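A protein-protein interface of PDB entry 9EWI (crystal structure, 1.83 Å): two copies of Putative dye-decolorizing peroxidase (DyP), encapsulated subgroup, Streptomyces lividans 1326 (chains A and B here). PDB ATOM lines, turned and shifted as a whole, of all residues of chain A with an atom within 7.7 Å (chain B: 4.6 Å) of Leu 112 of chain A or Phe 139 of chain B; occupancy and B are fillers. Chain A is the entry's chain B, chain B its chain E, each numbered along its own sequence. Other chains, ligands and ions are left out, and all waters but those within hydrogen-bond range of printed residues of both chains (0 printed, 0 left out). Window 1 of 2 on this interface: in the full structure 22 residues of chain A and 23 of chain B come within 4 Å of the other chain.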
ATOM      1  N   SER A  19      -6.589  32.346  11.163  1.00  0.00           N
ATOM      2  CA  SER A  19      -5.885  31.286  11.848  1.00  0.00           C
ATOM      3  C   SER A  19      -6.685  29.981  11.838  1.00  0.00           C
ATOM      4  O   SER A  19      -6.200  28.989  12.365  1.00  0.00           O
ATOM      5  CB  SER A  19      -5.562  31.747  13.230  1.00  0.00           C
ATOM      6  OG  SER A  19      -6.701  32.451  13.670  1.00  0.00           O
ATOM      7  N   ALA A  20      -7.878  29.958  11.221  1.00  0.00           N
ATOM      8  CA  ALA A  20      -8.628  28.712  11.162  1.00  0.00           C
ATOM      9  C   ALA A  20      -9.229  28.534   9.791  1.00  0.00           C
ATOM     10  O   ALA A  20      -9.562  29.526   9.145  1.00  0.00           O
ATOM     11  CB  ALA A  20      -9.730  28.697  12.179  1.00  0.00           C
ATOM     12  N   ALA A  21      -9.427  27.275   9.393  1.00  0.00           N
ATOM     13  CA  ALA A  21     -10.031  26.989   8.109  1.00  0.00           C
ATOM     14  C   ALA A  21     -10.732  25.646   8.140  1.00  0.00           C
ATOM     15  O   ALA A  21     -10.313  24.745   8.855  1.00  0.00           O
ATOM     16  CB  ALA A  21      -9.029  26.999   7.000  1.00  0.00           C
ATOM     17  N   ILE A  22     -11.812  25.551   7.346  1.00  0.00           N
ATOM     18  CA  ILE A  22     -12.376  24.272   6.985  1.00  0.00           C
ATOM     19  C   ILE A  22     -12.297  24.132   5.480  1.00  0.00           C
ATOM     20  O   ILE A  22     -12.739  25.013   4.760  1.00  0.00           O
ATOM     21  CB  ILE A  22     -13.794  24.096   7.517  1.00  0.00           C
ATOM     22  CG1 ILE A  22     -13.788  23.984   9.072  1.00  0.00           C
ATOM     23  CG2 ILE A  22     -14.412  22.850   6.870  1.00  0.00           C
ATOM     24  CD1 ILE A  22     -15.152  23.726   9.712  1.00  0.00           C
ATOM     25  N   LEU A  60     -14.734  36.007   8.595  1.00  0.00           N
ATOM     26  CA  LEU A  60     -15.273  34.812   7.969  1.00  0.00           C
ATOM     27  C   LEU A  60     -15.395  35.032   6.474  1.00  0.00           C
ATOM     28  O   LEU A  60     -15.891  36.037   6.067  1.00  0.00           O
ATOM     29  CB  LEU A  60     -16.620  34.438   8.567  1.00  0.00           C
ATOM     30  CG  LEU A  60     -17.324  33.258   7.908  1.00  0.00           C
ATOM     31  CD1 LEU A  60     -16.646  31.934   8.168  1.00  0.00           C
ATOM     32  CD2 LEU A  60     -18.729  33.183   8.424  1.00  0.00           C
ATOM     33  N   ILE A 107     -13.272  27.647   3.592  1.00  0.00           N
ATOM     34  CA  ILE A 107     -13.902  28.478   4.590  1.00  0.00           C
ATOM     35  C   ILE A 107     -12.831  28.918   5.571  1.00  0.00           C
ATOM     36  O   ILE A 107     -12.134  28.068   6.110  1.00  0.00           O
ATOM     37  CB  ILE A 107     -15.018  27.697   5.296  1.00  0.00           C
ATOM     38  CG1 ILE A 107     -16.063  27.190   4.261  1.00  0.00           C
ATOM     39  CG2 ILE A 107     -15.652  28.557   6.390  1.00  0.00           C
ATOM     40  CD1 ILE A 107     -17.061  26.182   4.806  1.00  0.00           C
ATOM     41  N   ARG A 108     -12.715  30.236   5.792  1.00  0.00           N
ATOM     42  CA  ARG A 108     -11.679  30.764   6.641  1.00  0.00           C
ATOM     43  C   ARG A 108     -12.281  31.726   7.646  1.00  0.00           C
ATOM     44  O   ARG A 108     -13.167  32.488   7.312  1.00  0.00           O
ATOM     45  CB  ARG A 108     -10.623  31.508   5.822  1.00  0.00           C
ATOM     46  CG  ARG A 108      -9.700  30.569   5.057  1.00  0.00           C
ATOM     47  CD  ARG A 108      -8.699  31.316   4.190  1.00  0.00           C
ATOM     48  NE  ARG A 108      -9.334  31.935   3.029  1.00  0.00           N
ATOM     49  CZ  ARG A 108      -8.668  32.384   1.968  1.00  0.00           C
ATOM     50  NH1 ARG A 108      -7.351  32.330   1.959  1.00  0.00           N
ATOM     51  NH2 ARG A 108      -9.298  32.854   0.914  1.00  0.00           N
ATOM     52  N   ALA A 109     -11.693  31.753   8.836  1.00  0.00           N
ATOM     53  CA  ALA A 109     -12.051  32.765   9.817  1.00  0.00           C
ATOM     54  C   ALA A 109     -10.976  32.886  10.895  1.00  0.00           C
ATOM     55  O   ALA A 109     -10.014  32.106  10.913  1.00  0.00           O
ATOM     56  CB  ALA A 109     -13.377  32.385  10.405  1.00  0.00           C
ATOM     57  N   SER A 110     -11.195  33.804  11.848  1.00  0.00           N
ATOM     58  CA  SER A 110     -10.287  33.906  12.972  1.00  0.00           C
ATOM     59  C   SER A 110     -10.540  32.810  13.995  1.00  0.00           C
ATOM     60  O   SER A 110      -9.698  32.588  14.845  1.00  0.00           O
ATOM     61  CB  SER A 110     -10.365  35.246  13.604  1.00  0.00           C
ATOM     62  OG  SER A 110     -11.649  35.454  14.160  1.00  0.00           O
ATOM     63  N   ARG A 111     -11.655  32.079  13.912  1.00  0.00           N
ATOM     64  CA  ARG A 111     -11.954  31.047  14.901  1.00  0.00           C
ATOM     65  C   ARG A 111     -12.664  29.884  14.224  1.00  0.00           C
ATOM     66  O   ARG A 111     -13.486  30.113  13.358  1.00  0.00           O
ATOM     67  CB  ARG A 111     -13.023  31.515  15.896  1.00  0.00           C
ATOM     68  CG  ARG A 111     -12.972  32.905  16.504  1.00  0.00           C
ATOM     69  CD  ARG A 111     -14.271  33.351  17.153  1.00  0.00           C
ATOM     70  NE  ARG A 111     -14.669  32.369  18.174  1.00  0.00           N
ATOM     71  CZ  ARG A 111     -14.493  32.356  19.488  1.00  0.00           C
ATOM     72  NH1 ARG A 111     -13.822  33.329  20.062  1.00  0.00           N
ATOM     73  NH2 ARG A 111     -14.969  31.369  20.238  1.00  0.00           N
ATOM     74  N   LEU A 112     -12.385  28.670  14.664  1.00  0.00           N
ATOM     75  CA  LEU A 112     -12.940  27.482  14.045  1.00  0.00           C
ATOM     76  C   LEU A 112     -14.474  27.413  14.092  1.00  0.00           C
ATOM     77  O   LEU A 112     -15.107  26.923  13.157  1.00  0.00           O
ATOM     78  CB  LEU A 112     -12.313  26.270  14.732  1.00  0.00           C
ATOM     79  CG  LEU A 112     -12.584  24.949  14.022  1.00  0.00           C
ATOM     80  CD1 LEU A 112     -12.032  24.992  12.605  1.00  0.00           C
ATOM     81  CD2 LEU A 112     -11.964  23.828  14.790  1.00  0.00           C
ATOM     82  N   ASP A 113     -15.081  27.924  15.174  1.00  0.00           N
ATOM     83  CA  ASP A 113     -16.520  27.814  15.346  1.00  0.00           C
ATOM     84  C   ASP A 113     -17.270  28.510  14.233  1.00  0.00           C
ATOM     85  O   ASP A 113     -18.277  28.017  13.803  1.00  0.00           O
ATOM     86  CB  ASP A 113     -16.998  28.361  16.681  1.00  0.00           C
ATOM     87  CG  ASP A 113     -16.513  29.764  17.010  1.00  0.00           C
ATOM     88  OD1 ASP A 113     -15.264  29.803  17.316  1.00  0.00           O
ATOM     89  OD2 ASP A 113     -17.378  30.737  16.924  1.00  0.00           O
ATOM     90  N   LEU A 114     -16.812  29.666  13.791  1.00  0.00           N
ATOM     91  CA  LEU A 114     -17.433  30.381  12.687  1.00  0.00           C
ATOM     92  C   LEU A 114     -17.339  29.577  11.396  1.00  0.00           C
ATOM     93  O   LEU A 114     -18.294  29.583  10.620  1.00  0.00           O
ATOM     94  CB  LEU A 114     -16.732  31.721  12.462  1.00  0.00           C
ATOM     95  CG  LEU A 114     -16.976  32.784  13.516  1.00  0.00           C
ATOM     96  CD1 LEU A 114     -16.235  34.032  13.155  1.00  0.00           C
ATOM     97  CD2 LEU A 114     -18.466  33.123  13.571  1.00  0.00           C
ATOM     98  N   CYS A 115     -16.170  28.954  11.159  1.00  0.00           N
ATOM     99  CA  CYS A 115     -15.994  28.068  10.025  1.00  0.00           C
ATOM    100  C   CYS A 115     -17.013  26.942  10.078  1.00  0.00           C
ATOM    101  O   CYS A 115     -17.669  26.627   9.072  1.00  0.00           O
ATOM    102  CB  CYS A 115     -14.594  27.493   9.982  1.00  0.00           C
ATOM    103  SG  CYS A 115     -13.337  28.758   9.694  1.00  0.00           S
ATOM    104  N   PHE A 116     -17.170  26.370  11.271  1.00  0.00           N
ATOM    105  CA  PHE A 116     -18.033  25.216  11.433  1.00  0.00           C
ATOM    106  C   PHE A 116     -19.487  25.639  11.260  1.00  0.00           C
ATOM    107  O   PHE A 116     -20.270  24.906  10.674  1.00  0.00           O
ATOM    108  CB  PHE A 116     -17.783  24.592  12.797  1.00  0.00           C
ATOM    109  CG  PHE A 116     -18.436  23.235  12.962  1.00  0.00           C
ATOM    110  CD1 PHE A 116     -17.781  22.073  12.562  1.00  0.00           C
ATOM    111  CD2 PHE A 116     -19.684  23.144  13.541  1.00  0.00           C
ATOM    112  CE1 PHE A 116     -18.394  20.842  12.693  1.00  0.00           C
ATOM    113  CE2 PHE A 116     -20.284  21.893  13.720  1.00  0.00           C
ATOM    114  CZ  PHE A 116     -19.652  20.752  13.278  1.00  0.00           C
ATOM    115  N   ALA A 117     -19.869  26.810  11.767  1.00  0.00           N
ATOM    116  CA  ALA A 117     -21.246  27.258  11.639  1.00  0.00           C
ATOM    117  C   ALA A 117     -21.616  27.426  10.172  1.00  0.00           C
ATOM    118  O   ALA A 117     -22.693  27.015   9.753  1.00  0.00           O
ATOM    119  CB  ALA A 117     -21.464  28.548  12.427  1.00  0.00           C
ATOM    120  N   LEU A 118     -20.702  28.026   9.379  1.00  0.00           N
ATOM    121  CA  LEU A 118     -20.986  28.219   7.964  1.00  0.00           C
ATOM    122  C   LEU A 118     -21.010  26.864   7.229  1.00  0.00           C
ATOM    123  O   LEU A 118     -21.893  26.614   6.406  1.00  0.00           O
ATOM    124  CB  LEU A 118     -20.003  29.206   7.354  1.00  0.00           C
ATOM    125  CG  LEU A 118     -20.205  29.416   5.837  1.00  0.00           C
ATOM    126  CD1 LEU A 118     -21.612  29.928   5.456  1.00  0.00           C
ATOM    127  CD2 LEU A 118     -19.192  30.369   5.272  1.00  0.00           C
ATOM    128  N   ALA A 119     -20.026  25.988   7.509  1.00  0.00           N
ATOM    129  CA  ALA A 119     -20.013  24.659   6.908  1.00  0.00           C
ATOM    130  C   ALA A 119     -21.311  23.895   7.187  1.00  0.00           C
ATOM    131  O   ALA A 119     -21.809  23.210   6.332  1.00  0.00           O
ATOM    132  CB  ALA A 119     -18.805  23.879   7.389  1.00  0.00           C
ATOM    133  N   THR A 120     -21.825  23.995   8.405  1.00  0.00           N
ATOM    134  CA  THR A 120     -23.059  23.342   8.809  1.00  0.00           C
ATOM    135  C   THR A 120     -24.214  23.843   7.947  1.00  0.00           C
ATOM    136  O   THR A 120     -25.015  23.047   7.485  1.00  0.00           O
ATOM    137  CB  THR A 120     -23.346  23.631  10.284  1.00  0.00           C
ATOM    138  OG1 THR A 120     -22.342  22.963  11.026  1.00  0.00           O
ATOM    139  CG2 THR A 120     -24.590  22.921  10.745  1.00  0.00           C
ATOM    140  N   VAL A 136     -11.330  18.844   6.318  1.00  0.00           N
ATOM    141  CA  VAL A 136     -10.145  19.090   7.111  1.00  0.00           C
ATOM    142  C   VAL A 136     -10.375  20.383   7.913  1.00  0.00           C
ATOM    143  O   VAL A 136     -10.827  21.400   7.369  1.00  0.00           O
ATOM    144  CB  VAL A 136      -8.903  19.187   6.200  1.00  0.00           C
ATOM    145  CG1 VAL A 136      -7.673  19.702   6.918  1.00  0.00           C
ATOM    146  CG2 VAL A 136      -8.564  17.873   5.574  1.00  0.00           C
ATOM    147  N   HIS A 137     -10.070  20.304   9.222  1.00  0.00           N
ATOM    148  CA  HIS A 137     -10.163  21.420  10.150  1.00  0.00           C
ATOM    149  C   HIS A 137      -8.739  21.855  10.393  1.00  0.00           C
ATOM    150  O   HIS A 137      -7.983  21.087  10.954  1.00  0.00           O
ATOM    151  CB  HIS A 137     -10.856  21.033  11.463  1.00  0.00           C
ATOM    152  CG  HIS A 137     -12.274  20.595  11.282  1.00  0.00           C
ATOM    153  ND1 HIS A 137     -13.097  20.317  12.351  1.00  0.00           N
ATOM    154  CD2 HIS A 137     -13.026  20.339  10.160  1.00  0.00           C
ATOM    155  CE1 HIS A 137     -14.281  19.935  11.876  1.00  0.00           C
ATOM    156  NE2 HIS A 137     -14.255  19.919  10.556  1.00  0.00           N
ATOM    157  N   GLY A 138      -8.391  23.030   9.845  1.00  0.00           N
ATOM    158  CA  GLY A 138      -7.033  23.515   9.862  1.00  0.00           C
ATOM    159  C   GLY A 138      -6.851  24.565  10.954  1.00  0.00           C
ATOM    160  O   GLY A 138      -7.801  25.291  11.267  1.00  0.00           O
ATOM    161  N   PHE A 139      -5.623  24.678  11.463  1.00  0.00           N
ATOM    162  CA  PHE A 139      -5.268  25.659  12.475  1.00  0.00           C
ATOM    163  C   PHE A 139      -3.843  26.147  12.217  1.00  0.00           C
ATOM    164  O   PHE A 139      -2.960  25.359  11.984  1.00  0.00           O
ATOM    165  CB  PHE A 139      -5.367  25.049  13.868  1.00  0.00           C
ATOM    166  CG  PHE A 139      -4.743  23.669  14.029  1.00  0.00           C
ATOM    167  CD1 PHE A 139      -3.401  23.529  14.337  1.00  0.00           C
ATOM    168  CD2 PHE A 139      -5.497  22.519  13.882  1.00  0.00           C
ATOM    169  CE1 PHE A 139      -2.825  22.269  14.472  1.00  0.00           C
ATOM    170  CE2 PHE A 139      -4.945  21.272  14.027  1.00  0.00           C
ATOM    171  CZ  PHE A 139      -3.605  21.148  14.320  1.00  0.00           C
ATOM    172  N   SER B  19     -11.283  29.119  24.562  1.00  0.00           N
ATOM    173  CA  SER B  19     -12.222  28.836  23.496  1.00  0.00           C
ATOM    174  C   SER B  19     -11.842  27.567  22.733  1.00  0.00           C
ATOM    175  O   SER B  19     -12.538  27.159  21.795  1.00  0.00           O
ATOM    176  CB  SER B  19     -12.299  30.037  22.598  1.00  0.00           C
ATOM    177  OG  SER B  19     -10.996  30.570  22.582  1.00  0.00           O
ATOM    178  N   LEU B 112      -6.499  26.489  19.108  1.00  0.00           N
ATOM    179  CA  LEU B 112      -6.368  25.053  19.005  1.00  0.00           C
ATOM    180  C   LEU B 112      -4.913  24.600  18.823  1.00  0.00           C
ATOM    181  O   LEU B 112      -4.505  23.525  19.315  1.00  0.00           O
ATOM    182  CB  LEU B 112      -7.235  24.599  17.850  1.00  0.00           C
ATOM    183  CG  LEU B 112      -7.407  23.082  17.750  1.00  0.00           C
ATOM    184  CD1 LEU B 112      -7.924  22.504  19.048  1.00  0.00           C
ATOM    185  CD2 LEU B 112      -8.410  22.751  16.662  1.00  0.00           C
ATOM    186  N   HIS B 137     -11.442  17.452  19.567  1.00  0.00           N
ATOM    187  CA  HIS B 137     -10.994  18.814  19.367  1.00  0.00           C
ATOM    188  C   HIS B 137     -12.222  19.680  19.517  1.00  0.00           C
ATOM    189  O   HIS B 137     -13.103  19.591  18.684  1.00  0.00           O
ATOM    190  CB  HIS B 137     -10.370  18.991  17.970  1.00  0.00           C
ATOM    191  CG  HIS B 137      -9.119  18.197  17.779  1.00  0.00           C
ATOM    192  ND1 HIS B 137      -8.356  18.305  16.646  1.00  0.00           N
ATOM    193  CD2 HIS B 137      -8.501  17.249  18.555  1.00  0.00           C
ATOM    194  CE1 HIS B 137      -7.361  17.425  16.712  1.00  0.00           C
ATOM    195  NE2 HIS B 137      -7.429  16.773  17.880  1.00  0.00           N
ATOM    196  N   GLY B 138     -12.282  20.445  20.604  1.00  0.00           N
ATOM    197  CA  GLY B 138     -13.468  21.195  20.954  1.00  0.00           C
ATOM    198  C   GLY B 138     -13.276  22.674  20.619  1.00  0.00           C
ATOM    199  O   GLY B 138     -12.156  23.163  20.675  1.00  0.00           O
ATOM    200  N   PHE B 139     -14.383  23.372  20.341  1.00  0.00           N
ATOM    201  CA  PHE B 139     -14.374  24.801  20.048  1.00  0.00           C
ATOM    202  C   PHE B 139     -15.631  25.445  20.617  1.00  0.00           C
ATOM    203  O   PHE B 139     -16.720  24.950  20.452  1.00  0.00           O
ATOM    204  CB  PHE B 139     -14.294  25.028  18.531  1.00  0.00           C
ATOM    205  CG  PHE B 139     -15.271  24.201  17.706  1.00  0.00           C
ATOM    206  CD1 PHE B 139     -16.563  24.632  17.474  1.00  0.00           C
ATOM    207  CD2 PHE B 139     -14.871  22.991  17.150  1.00  0.00           C
ATOM    208  CE1 PHE B 139     -17.461  23.863  16.753  1.00  0.00           C
ATOM    209  CE2 PHE B 139     -15.759  22.241  16.394  1.00  0.00           C
ATOM    210  CZ  PHE B 139     -17.060  22.689  16.199  1.00  0.00           C
ATOM    211  N   LYS B 140     -15.477  26.564  21.301  1.00  0.00           N
ATOM    212  CA  LYS B 140     -16.614  27.271  21.860  1.00  0.00           C
ATOM    213  C   LYS B 140     -17.159  28.189  20.776  1.00  0.00           C
ATOM    214  O   LYS B 140     -16.392  28.719  20.009  1.00  0.00           O
ATOM    215  CB  LYS B 140     -16.192  28.051  23.107  1.00  0.00           C
ATOM    216  CG  LYS B 140     -17.304  28.225  24.137  1.00  0.00           C
ATOM    217  CD  LYS B 140     -17.711  26.976  24.944  1.00  0.00           C
ATOM    218  CE  LYS B 140     -19.155  26.937  25.505  1.00  0.00           C
ATOM    219  NZ  LYS B 140     -19.249  27.655  26.782  1.00  0.00           N
ATOM    220  N   TYR B 141     -18.480  28.324  20.687  1.00  0.00           N
ATOM    221  CA  TYR B 141     -19.123  29.333  19.852  1.00  0.00           C
ATOM    222  C   TYR B 141     -18.943  30.725  20.440  1.00  0.00           C
ATOM    223  O   TYR B 141     -18.588  30.858  21.612  1.00  0.00           O
ATOM    224  CB  TYR B 141     -20.608  29.073  19.671  1.00  0.00           C
ATOM    225  CG  TYR B 141     -20.850  27.915  18.717  1.00  0.00           C
ATOM    226  CD1 TYR B 141     -20.794  26.625  19.159  1.00  0.00           C
ATOM    227  CD2 TYR B 141     -21.103  28.111  17.375  1.00  0.00           C
ATOM    228  CE1 TYR B 141     -21.008  25.558  18.304  1.00  0.00           C
ATOM    229  CE2 TYR B 141     -21.342  27.072  16.512  1.00  0.00           C
ATOM    230  CZ  TYR B 141     -21.263  25.791  16.975  1.00  0.00           C
ATOM    231  OH  TYR B 141     -21.453  24.731  16.177  1.00  0.00           O
ATOM    232  N   MET B 246     -17.746  21.521  25.873  1.00  0.00           N
ATOM    233  CA  MET B 246     -17.221  22.012  24.611  1.00  0.00           C
ATOM    234  C   MET B 246     -17.941  21.348  23.451  1.00  0.00           C
ATOM    235  O   MET B 246     -18.049  20.127  23.382  1.00  0.00           O
ATOM    236  CB  MET B 246     -15.736  21.654  24.431  1.00  0.00           C
ATOM    237  CG  MET B 246     -14.814  22.397  25.385  1.00  0.00           C
ATOM    238  SD  MET B 246     -14.861  24.199  25.249  1.00  0.00           S
ATOM    239  CE  MET B 246     -13.862  24.345  23.769  1.00  0.00           C
ATOM    240  N   PRO B 247     -18.435  22.127  22.480  1.00  0.00           N
ATOM    241  CA  PRO B 247     -18.917  21.572  21.222  1.00  0.00           C
ATOM    242  C   PRO B 247     -17.796  20.917  20.439  1.00  0.00           C
ATOM    243  O   PRO B 247     -16.624  21.284  20.503  1.00  0.00           O
ATOM    244  CB  PRO B 247     -19.406  22.812  20.474  1.00  0.00           C
ATOM    245  CG  PRO B 247     -19.605  23.855  21.529  1.00  0.00           C
ATOM    246  CD  PRO B 247     -18.604  23.576  22.596  1.00  0.00           C
ATOM    247  N   PHE B 248     -18.189  19.978  19.600  1.00  0.00           N
ATOM    248  CA  PHE B 248     -17.277  19.387  18.638  1.00  0.00           C
ATOM    249  C   PHE B 248     -18.152  18.831  17.522  1.00  0.00           C
ATOM    250  O   PHE B 248     -19.351  18.682  17.698  1.00  0.00           O
ATOM    251  CB  PHE B 248     -16.407  18.287  19.272  1.00  0.00           C
ATOM    252  CG  PHE B 248     -17.219  17.047  19.649  1.00  0.00           C
ATOM    253  CD1 PHE B 248     -17.860  16.970  20.878  1.00  0.00           C
ATOM    254  CD2 PHE B 248     -17.363  15.985  18.768  1.00  0.00           C
ATOM    255  CE1 PHE B 248     -18.589  15.847  21.216  1.00  0.00           C
ATOM    256  CE2 PHE B 248     -18.099  14.868  19.105  1.00  0.00           C
ATOM    257  CZ  PHE B 248     -18.712  14.808  20.324  1.00  0.00           C
ATOM    258  N   GLY B 249     -17.506  18.512  16.405  1.00  0.00           N
ATOM    259  CA  GLY B 249     -18.215  17.789  15.395  1.00  0.00           C
ATOM    260  C   GLY B 249     -17.458  17.615  14.087  1.00  0.00           C
ATOM    261  O   GLY B 249     -16.317  18.012  13.902  1.00  0.00           O
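The guanidinium group (NH2) of Arg 111 of chain A sits at hydrogen-bond distance from the backbone carbonyl oxygen (O) of Lys 140 of chain B, 3.0 Å away.
The side-chain carboxylate of Asp 113 of chain A sits close to the backbone carbonyl oxygen of Lys 140 of chain B (3.1 Å).
OD1 of Asp 113 of chain A is in salt-bridge range of NE of Arg 111 of chain A, at 2.8 Å.
The backbone carbonyl oxygen (O) of Phe 116 of chain A is in hydrogen-bond range of the side-chain hydroxyl (OG1) of Thr 120 of chain A (2.9 Å).
The backbone carbonyl oxygen (O) of Ser 19 of chain B is in hydrogen-bond range of the backbone NH (N) of Lys 140 of chain B (3.0 Å).
O of Pro 247 of chain B is in hydrogen-bond range of N of Phe 139 of chain B.
Ser 19 of chain B touches Arg 111 of chain A (CB to NH2, 3.8 Å).
Tyr 141 of chain B touches Arg 111 of chain A (O to NH2, 3.9 Å).
CD2 of Leu 112 of chain A touches CD2 of Phe 139 of chain B (3.8 Å).
Asp 113 of chain A touches Phe 139 of chain B.
CA of Tyr 141 of chain B touches OD2 of Asp 113 of chain A, 3.7 Å away.
CG of Phe 116 of chain A touches CZ of Phe 139 of chain B, at 3.6 Å.
Phe 116 of chain A touches Tyr 141 of chain B (CD2 to OH, 3.5 Å).
CE1 of Phe 116 of chain A touches C of Gly 249 of chain B, 3.6 Å away.
His 137 of chain A touches Gly 249 of chain B.
Of the printed residues of chain B, Arg 111 of chain A touches Ser 19 (3.8 Å), Lys 140 (3.0 Å) and Tyr 141 (3.9 Å).
Of chain B, only Phe 139 (3.8 Å) comes within 4 Å of Leu 112 of chain A.
Printed residues of chain B within 4 Å of Phe 116 of chain A: Phe 139 (3.6 Å), Tyr 141 (3.5 Å) and Gly 249 (3.6 Å).
Of the printed residues of chain B, His 137 of chain A touches Gly 249 (3.5 Å).
Gly 138 of chain B touches none of the printed residues of chain A.
Phe 139 of chain B touches just these residues of chain A: Leu 112, Asp 113 and Phe 116.
Of the printed residues of chain A, Tyr 141 of chain B touches Arg 111, Asp 113 and Phe 116.
Pro 247 of chain B touches none of the printed residues of chain A.
The nearest residue of chain B that does not touch Leu 112 of chain A is Leu 112 of chain B (4.2 Å).
The nearest printed residue of chain B that does not touch His 137 of chain A is Phe 139 of chain B (5.2 Å).
Of the 23 printed residues of chain A, 5 touch a printed residue of chain B.
Hydrophobic or aromatic side chains of chain A within 4 Å of the printed part of chain B: Leu 112, Phe 116 and His 137.
Of the 11 printed residues of chain B, 5 touch a printed residue of chain A.
Hydrophobic or aromatic side chains of chain B that line the printed part of chain A: Phe 139 and Tyr 141.
Along chain B the printed residues that touch a printed residue of chain A span positions 19 to 249.
Leu 112 of chain A touches Phe 139 of chain B, but with the chains exchanged Phe 139 of chain A does not touch Leu 112 of chain B (4.03 Å).
Positions printed for both chains: 19, 112, 137, 138 and 139.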
